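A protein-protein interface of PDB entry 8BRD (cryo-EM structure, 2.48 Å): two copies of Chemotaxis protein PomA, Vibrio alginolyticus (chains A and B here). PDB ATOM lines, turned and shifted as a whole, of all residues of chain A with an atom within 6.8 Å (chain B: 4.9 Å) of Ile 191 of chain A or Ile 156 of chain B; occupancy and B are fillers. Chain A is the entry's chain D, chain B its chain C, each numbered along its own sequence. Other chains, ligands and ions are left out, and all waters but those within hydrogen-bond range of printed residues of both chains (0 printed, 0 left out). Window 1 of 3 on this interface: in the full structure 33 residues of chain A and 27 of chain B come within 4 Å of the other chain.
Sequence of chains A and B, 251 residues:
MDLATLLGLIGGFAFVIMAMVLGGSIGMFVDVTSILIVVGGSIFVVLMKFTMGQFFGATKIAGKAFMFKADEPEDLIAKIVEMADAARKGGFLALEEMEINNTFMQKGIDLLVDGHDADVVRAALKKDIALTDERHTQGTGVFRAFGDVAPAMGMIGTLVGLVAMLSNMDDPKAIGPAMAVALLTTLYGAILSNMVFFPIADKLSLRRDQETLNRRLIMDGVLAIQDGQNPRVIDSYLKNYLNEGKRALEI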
ATOM      1  N   VAL A  16     -19.934   5.768  -0.581  1.00  0.00           N
ATOM      2  CA  VAL A  16     -21.206   5.044  -0.572  1.00  0.00           C
ATOM      3  C   VAL A  16     -21.147   3.863   0.394  1.00  0.00           C
ATOM      4  O   VAL A  16     -22.072   3.643   1.192  1.00  0.00           O
ATOM      5  CB  VAL A  16     -21.576   4.590  -1.994  1.00  0.00           C
ATOM      6  CG1 VAL A  16     -22.901   3.851  -1.982  1.00  0.00           C
ATOM      7  CG2 VAL A  16     -21.651   5.783  -2.923  1.00  0.00           C
ATOM      8  N   MET A  20     -23.277   3.227   3.868  1.00  0.00           N
ATOM      9  CA  MET A  20     -24.060   2.026   4.156  1.00  0.00           C
ATOM     10  C   MET A  20     -23.625   1.380   5.467  1.00  0.00           C
ATOM     11  O   MET A  20     -24.461   0.897   6.239  1.00  0.00           O
ATOM     12  CB  MET A  20     -23.945   1.029   3.004  1.00  0.00           C
ATOM     13  CG  MET A  20     -24.809   1.363   1.804  1.00  0.00           C
ATOM     14  SD  MET A  20     -25.528  -0.108   1.052  1.00  0.00           S
ATOM     15  CE  MET A  20     -25.295   0.258  -0.686  1.00  0.00           C
ATOM     16  N   THR A 186     -35.326  -4.390  -5.273  1.00  0.00           N
ATOM     17  CA  THR A 186     -35.489  -3.063  -5.859  1.00  0.00           C
ATOM     18  C   THR A 186     -34.233  -2.221  -5.670  1.00  0.00           C
ATOM     19  O   THR A 186     -33.825  -1.483  -6.573  1.00  0.00           O
ATOM     20  CB  THR A 186     -36.707  -2.379  -5.240  1.00  0.00           C
ATOM     21  OG1 THR A 186     -37.883  -3.127  -5.560  1.00  0.00           O
ATOM     22  CG2 THR A 186     -36.864  -0.963  -5.750  1.00  0.00           C
ATOM     23  N   LEU A 187     -33.602  -2.332  -4.502  1.00  0.00           N
ATOM     24  CA  LEU A 187     -32.357  -1.615  -4.251  1.00  0.00           C
ATOM     25  C   LEU A 187     -31.267  -2.035  -5.233  1.00  0.00           C
ATOM     26  O   LEU A 187     -30.585  -1.189  -5.818  1.00  0.00           O
ATOM     27  CB  LEU A 187     -31.904  -1.847  -2.807  1.00  0.00           C
ATOM     28  CG  LEU A 187     -30.545  -1.275  -2.395  1.00  0.00           C
ATOM     29  CD1 LEU A 187     -30.494   0.222  -2.609  1.00  0.00           C
ATOM     30  CD2 LEU A 187     -30.247  -1.613  -0.954  1.00  0.00           C
ATOM     31  N   TYR A 188     -31.096  -3.345  -5.430  1.00  0.00           N
ATOM     32  CA  TYR A 188     -30.083  -3.831  -6.366  1.00  0.00           C
ATOM     33  C   TYR A 188     -30.396  -3.413  -7.793  1.00  0.00           C
ATOM     34  O   TYR A 188     -29.495  -3.031  -8.545  1.00  0.00           O
ATOM     35  CB  TYR A 188     -29.956  -5.351  -6.296  1.00  0.00           C
ATOM     36  CG  TYR A 188     -29.469  -5.897  -4.982  1.00  0.00           C
ATOM     37  CD1 TYR A 188     -28.814  -5.091  -4.069  1.00  0.00           C
ATOM     38  CD2 TYR A 188     -29.659  -7.229  -4.661  1.00  0.00           C
ATOM     39  CE1 TYR A 188     -28.374  -5.595  -2.872  1.00  0.00           C
ATOM     40  CE2 TYR A 188     -29.220  -7.742  -3.469  1.00  0.00           C
ATOM     41  CZ  TYR A 188     -28.578  -6.923  -2.579  1.00  0.00           C
ATOM     42  OH  TYR A 188     -28.140  -7.436  -1.387  1.00  0.00           O
ATOM     43  N   GLY A 189     -31.665  -3.500  -8.190  1.00  0.00           N
ATOM     44  CA  GLY A 189     -32.038  -3.062  -9.522  1.00  0.00           C
ATOM     45  C   GLY A 189     -31.745  -1.595  -9.754  1.00  0.00           C
ATOM     46  O   GLY A 189     -31.225  -1.216 -10.804  1.00  0.00           O
ATOM     47  N   ALA A 190     -32.051  -0.753  -8.765  1.00  0.00           N
ATOM     48  CA  ALA A 190     -31.780   0.676  -8.877  1.00  0.00           C
ATOM     49  C   ALA A 190     -30.284   0.960  -8.924  1.00  0.00           C
ATOM     50  O   ALA A 190     -29.828   1.793  -9.715  1.00  0.00           O
ATOM     51  CB  ALA A 190     -32.424   1.418  -7.713  1.00  0.00           C
ATOM     52  N   ILE A 191     -29.506   0.286  -8.076  1.00  0.00           N
ATOM     53  CA  ILE A 191     -28.064   0.510  -8.061  1.00  0.00           C
ATOM     54  C   ILE A 191     -27.452   0.103  -9.394  1.00  0.00           C
ATOM     55  O   ILE A 191     -26.665   0.845  -9.987  1.00  0.00           O
ATOM     56  CB  ILE A 191     -27.413  -0.247  -6.889  1.00  0.00           C
ATOM     57  CG1 ILE A 191     -27.717   0.449  -5.569  1.00  0.00           C
ATOM     58  CG2 ILE A 191     -25.917  -0.344  -7.085  1.00  0.00           C
ATOM     59  CD1 ILE A 191     -27.303  -0.348  -4.367  1.00  0.00           C
ATOM     60  N   LEU A 192     -27.819  -1.078  -9.894  1.00  0.00           N
ATOM     61  CA  LEU A 192     -27.272  -1.542 -11.163  1.00  0.00           C
ATOM     62  C   LEU A 192     -27.710  -0.649 -12.315  1.00  0.00           C
ATOM     63  O   LEU A 192     -26.923  -0.367 -13.223  1.00  0.00           O
ATOM     64  CB  LEU A 192     -27.684  -2.991 -11.405  1.00  0.00           C
ATOM     65  CG  LEU A 192     -26.998  -4.015 -10.504  1.00  0.00           C
ATOM     66  CD1 LEU A 192     -27.508  -5.410 -10.792  1.00  0.00           C
ATOM     67  CD2 LEU A 192     -25.497  -3.947 -10.682  1.00  0.00           C
ATOM     68  N   SER A 193     -28.961  -0.191 -12.292  1.00  0.00           N
ATOM     69  CA  SER A 193     -29.453   0.679 -13.351  1.00  0.00           C
ATOM     70  C   SER A 193     -28.720   2.015 -13.367  1.00  0.00           C
ATOM     71  O   SER A 193     -28.199   2.432 -14.406  1.00  0.00           O
ATOM     72  CB  SER A 193     -30.955   0.892 -13.174  1.00  0.00           C
ATOM     73  OG  SER A 193     -31.458   1.830 -14.101  1.00  0.00           O
ATOM     74  N   ASN A 194     -28.650   2.692 -12.220  1.00  0.00           N
ATOM     75  CA  ASN A 194     -28.235   4.087 -12.195  1.00  0.00           C
ATOM     76  C   ASN A 194     -26.758   4.289 -11.898  1.00  0.00           C
ATOM     77  O   ASN A 194     -26.243   5.386 -12.129  1.00  0.00           O
ATOM     78  CB  ASN A 194     -29.061   4.860 -11.167  1.00  0.00           C
ATOM     79  CG  ASN A 194     -30.511   4.985 -11.567  1.00  0.00           C
ATOM     80  OD1 ASN A 194     -30.824   5.359 -12.695  1.00  0.00           O
ATOM     81  ND2 ASN A 194     -31.408   4.675 -10.643  1.00  0.00           N
ATOM     82  N   MET A 195     -26.061   3.272 -11.402  1.00  0.00           N
ATOM     83  CA  MET A 195     -24.655   3.398 -11.061  1.00  0.00           C
ATOM     84  C   MET A 195     -23.740   2.562 -11.937  1.00  0.00           C
ATOM     85  O   MET A 195     -22.529   2.801 -11.938  1.00  0.00           O
ATOM     86  CB  MET A 195     -24.427   3.012  -9.591  1.00  0.00           C
ATOM     87  CG  MET A 195     -25.054   3.957  -8.587  1.00  0.00           C
ATOM     88  SD  MET A 195     -24.597   3.544  -6.896  1.00  0.00           S
ATOM     89  CE  MET A 195     -23.270   4.709  -6.611  1.00  0.00           C
ATOM     90  N   VAL A 196     -24.273   1.592 -12.676  1.00  0.00           N
ATOM     91  CA  VAL A 196     -23.431   0.703 -13.466  1.00  0.00           C
ATOM     92  C   VAL A 196     -23.822   0.757 -14.937  1.00  0.00           C
ATOM     93  O   VAL A 196     -23.010   1.128 -15.788  1.00  0.00           O
ATOM     94  CB  VAL A 196     -23.500  -0.740 -12.936  1.00  0.00           C
ATOM     95  CG1 VAL A 196     -22.641  -1.653 -13.788  1.00  0.00           C
ATOM     96  CG2 VAL A 196     -23.061  -0.791 -11.485  1.00  0.00           C
ATOM     97  N   PHE A 197     -25.068   0.404 -15.247  1.00  0.00           N
ATOM     98  CA  PHE A 197     -25.446   0.168 -16.637  1.00  0.00           C
ATOM     99  C   PHE A 197     -25.683   1.470 -17.396  1.00  0.00           C
ATOM    100  O   PHE A 197     -25.131   1.666 -18.482  1.00  0.00           O
ATOM    101  CB  PHE A 197     -26.683  -0.727 -16.692  1.00  0.00           C
ATOM    102  CG  PHE A 197     -26.439  -2.114 -16.185  1.00  0.00           C
ATOM    103  CD1 PHE A 197     -25.341  -2.835 -16.614  1.00  0.00           C
ATOM    104  CD2 PHE A 197     -27.295  -2.691 -15.266  1.00  0.00           C
ATOM    105  CE1 PHE A 197     -25.107  -4.105 -16.146  1.00  0.00           C
ATOM    106  CE2 PHE A 197     -27.065  -3.962 -14.794  1.00  0.00           C
ATOM    107  CZ  PHE A 197     -25.967  -4.669 -15.233  1.00  0.00           C
ATOM    108  N   PRO A 199     -24.627   4.603 -16.527  1.00  0.00           N
ATOM    109  CA  PRO A 199     -23.334   5.284 -16.702  1.00  0.00           C
ATOM    110  C   PRO A 199     -22.454   4.678 -17.783  1.00  0.00           C
ATOM    111  O   PRO A 199     -21.801   5.424 -18.517  1.00  0.00           O
ATOM    112  CB  PRO A 199     -22.702   5.161 -15.311  1.00  0.00           C
ATOM    113  CG  PRO A 199     -23.845   5.135 -14.399  1.00  0.00           C
ATOM    114  CD  PRO A 199     -24.914   4.361 -15.101  1.00  0.00           C
ATOM    115  N   ALA B 152     -31.455  10.227  -8.715  1.00  0.00           N
ATOM    116  CA  ALA B 152     -31.343   8.772  -8.745  1.00  0.00           C
ATOM    117  C   ALA B 152     -30.578   8.261  -7.530  1.00  0.00           C
ATOM    118  O   ALA B 152     -30.977   7.282  -6.891  1.00  0.00           O
ATOM    119  CB  ALA B 152     -30.668   8.325 -10.040  1.00  0.00           C
ATOM    120  N   MET B 153     -29.476   8.931  -7.188  1.00  0.00           N
ATOM    121  CA  MET B 153     -28.739   8.581  -5.980  1.00  0.00           C
ATOM    122  C   MET B 153     -29.563   8.828  -4.728  1.00  0.00           C
ATOM    123  O   MET B 153     -29.448   8.080  -3.754  1.00  0.00           O
ATOM    124  CB  MET B 153     -27.429   9.370  -5.916  1.00  0.00           C
ATOM    125  CG  MET B 153     -26.339   8.867  -6.848  1.00  0.00           C
ATOM    126  SD  MET B 153     -26.086   7.077  -6.890  1.00  0.00           S
ATOM    127  CE  MET B 153     -26.002   6.670  -5.149  1.00  0.00           C
ATOM    128  N   GLY B 154     -30.391   9.872  -4.731  1.00  0.00           N
ATOM    129  CA  GLY B 154     -31.254  10.124  -3.593  1.00  0.00           C
ATOM    130  C   GLY B 154     -32.303   9.049  -3.415  1.00  0.00           C
ATOM    131  O   GLY B 154     -32.613   8.655  -2.293  1.00  0.00           O
ATOM    132  N   MET B 155     -32.857   8.552  -4.520  1.00  0.00           N
ATOM    133  CA  MET B 155     -33.815   7.458  -4.425  1.00  0.00           C
ATOM    134  C   MET B 155     -33.129   6.162  -4.001  1.00  0.00           C
ATOM    135  O   MET B 155     -33.704   5.370  -3.249  1.00  0.00           O
ATOM    136  CB  MET B 155     -34.560   7.301  -5.753  1.00  0.00           C
ATOM    137  CG  MET B 155     -35.583   6.176  -5.780  1.00  0.00           C
ATOM    138  SD  MET B 155     -35.718   5.418  -7.402  1.00  0.00           S
ATOM    139  CE  MET B 155     -34.308   4.330  -7.366  1.00  0.00           C
ATOM    140  N   ILE B 156     -31.885   5.947  -4.439  1.00  0.00           N
ATOM    141  CA  ILE B 156     -31.119   4.801  -3.951  1.00  0.00           C
ATOM    142  C   ILE B 156     -30.902   4.900  -2.445  1.00  0.00           C
ATOM    143  O   ILE B 156     -31.090   3.922  -1.707  1.00  0.00           O
ATOM    144  CB  ILE B 156     -29.780   4.689  -4.703  1.00  0.00           C
ATOM    145  CG1 ILE B 156     -29.998   4.171  -6.125  1.00  0.00           C
ATOM    146  CG2 ILE B 156     -28.807   3.804  -3.933  1.00  0.00           C
ATOM    147  CD1 ILE B 156     -28.782   4.277  -7.013  1.00  0.00           C
ATOM    148  N   GLY B 157     -30.502   6.080  -1.965  1.00  0.00           N
ATOM    149  CA  GLY B 157     -30.305   6.273  -0.539  1.00  0.00           C
ATOM    150  C   GLY B 157     -31.584   6.155   0.259  1.00  0.00           C
ATOM    151  O   GLY B 157     -31.570   5.671   1.391  1.00  0.00           O
ATOM    152  N   THR B 158     -32.705   6.596  -0.311  1.00  0.00           N
ATOM    153  CA  THR B 158     -33.992   6.414   0.350  1.00  0.00           C
ATOM    154  C   THR B 158     -34.370   4.940   0.415  1.00  0.00           C
ATOM    155  O   THR B 158     -34.939   4.489   1.409  1.00  0.00           O
ATOM    156  CB  THR B 158     -35.070   7.238  -0.363  1.00  0.00           C
ATOM    157  OG1 THR B 158     -34.891   8.620  -0.038  1.00  0.00           O
ATOM    158  CG2 THR B 158     -36.468   6.820   0.071  1.00  0.00           C
ATOM    159  N   LEU B 159     -34.050   4.169  -0.625  1.00  0.00           N
ATOM    160  CA  LEU B 159     -34.235   2.720  -0.557  1.00  0.00           C
ATOM    161  C   LEU B 159     -33.392   2.107   0.554  1.00  0.00           C
ATOM    162  O   LEU B 159     -33.865   1.241   1.301  1.00  0.00           O
ATOM    163  CB  LEU B 159     -33.878   2.082  -1.899  1.00  0.00           C
ATOM    164  CG  LEU B 159     -34.995   1.939  -2.927  1.00  0.00           C
ATOM    165  CD1 LEU B 159     -34.411   1.787  -4.322  1.00  0.00           C
ATOM    166  CD2 LEU B 159     -35.877   0.762  -2.573  1.00  0.00           C
ATOM    167  N   VAL B 160     -32.139   2.546   0.673  1.00  0.00           N
ATOM    168  CA  VAL B 160     -31.274   2.090   1.758  1.00  0.00           C
ATOM    169  C   VAL B 160     -31.895   2.417   3.112  1.00  0.00           C
ATOM    170  O   VAL B 160     -31.940   1.571   4.019  1.00  0.00           O
ATOM    171  CB  VAL B 160     -29.873   2.718   1.609  1.00  0.00           C
ATOM    172  CG1 VAL B 160     -29.041   2.499   2.859  1.00  0.00           C
ATOM    173  CG2 VAL B 160     -29.167   2.161   0.391  1.00  0.00           C
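Among the printed residues, merely in contact across the chains: Ala 190 of chain A with Met 155 of chain B, Met 195 of chain A with Met 153 of chain B, Asn 194 of chain A with Ala 152 of chain B, Thr 186 of chain A with Leu 159 of chain B, Leu 187 of chain A with Val 160 of chain B, Ala 190 of chain A with Ile 156 of chain B, Leu 187 of chain A with Ile 156 of chain B, Ile 191 of chain A with Ile 156 of chain B, Leu 187 of chain A with Leu 159 of chain B and Ala 190 of chain A with Leu 159 of chain B.
Ile 191 of chain A touches just one residue of chain B: Ile 156. Ile 156 of chain B touches just these residues of chain A: Leu 187 (3.9 Å), Ala 190 (3.8 Å) and Ile 191 (3.9 Å). Of the printed residues of chain B, Thr 186 of chain A touches Leu 159. Printed residues of chain A within 4 Å of Met 153 of chain B: Met 195. Printed residues of chain A within 4 Å of Val 160 of chain B: Leu 187 (3.8 Å). Of the printed residues of chain B, Met 195 of chain A touches Met 153.
Of the 15 printed residues of chain A, 6 touch a printed residue of chain B. Hydrophobic or aromatic side chains of chain A that line the printed part of chain B: Leu 187, Ala 190, Ile 191 and Met 195. Of the 9 printed residues of chain B, 6 touch a printed residue of chain A. Hydrophobic or aromatic side chains of chain B within 4 Å of the printed part of chain A: Ala 152, Met 153, Met 155, Ile 156, Leu 159 and Val 160. Along chain B the printed residues that touch a printed residue of chain A span positions 152 to 160. Among the printed residues, 10 pairs touch across the chains. Among the printed residues, no Asp or Glu carboxylate lies within 4 Å of a Lys or Arg side-chain nitrogen of the other chain.
No position is printed for both chains. Of the 10 pairs that touch across the chains among the printed residues, none has its exchanged pair printed and touching as well.
The backbone carbonyl oxygen of Ala 190 of chain A lies within hydrogen-bond range of the side-chain amide nitrogen of Asn 194 of chain A (3.4 Å).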
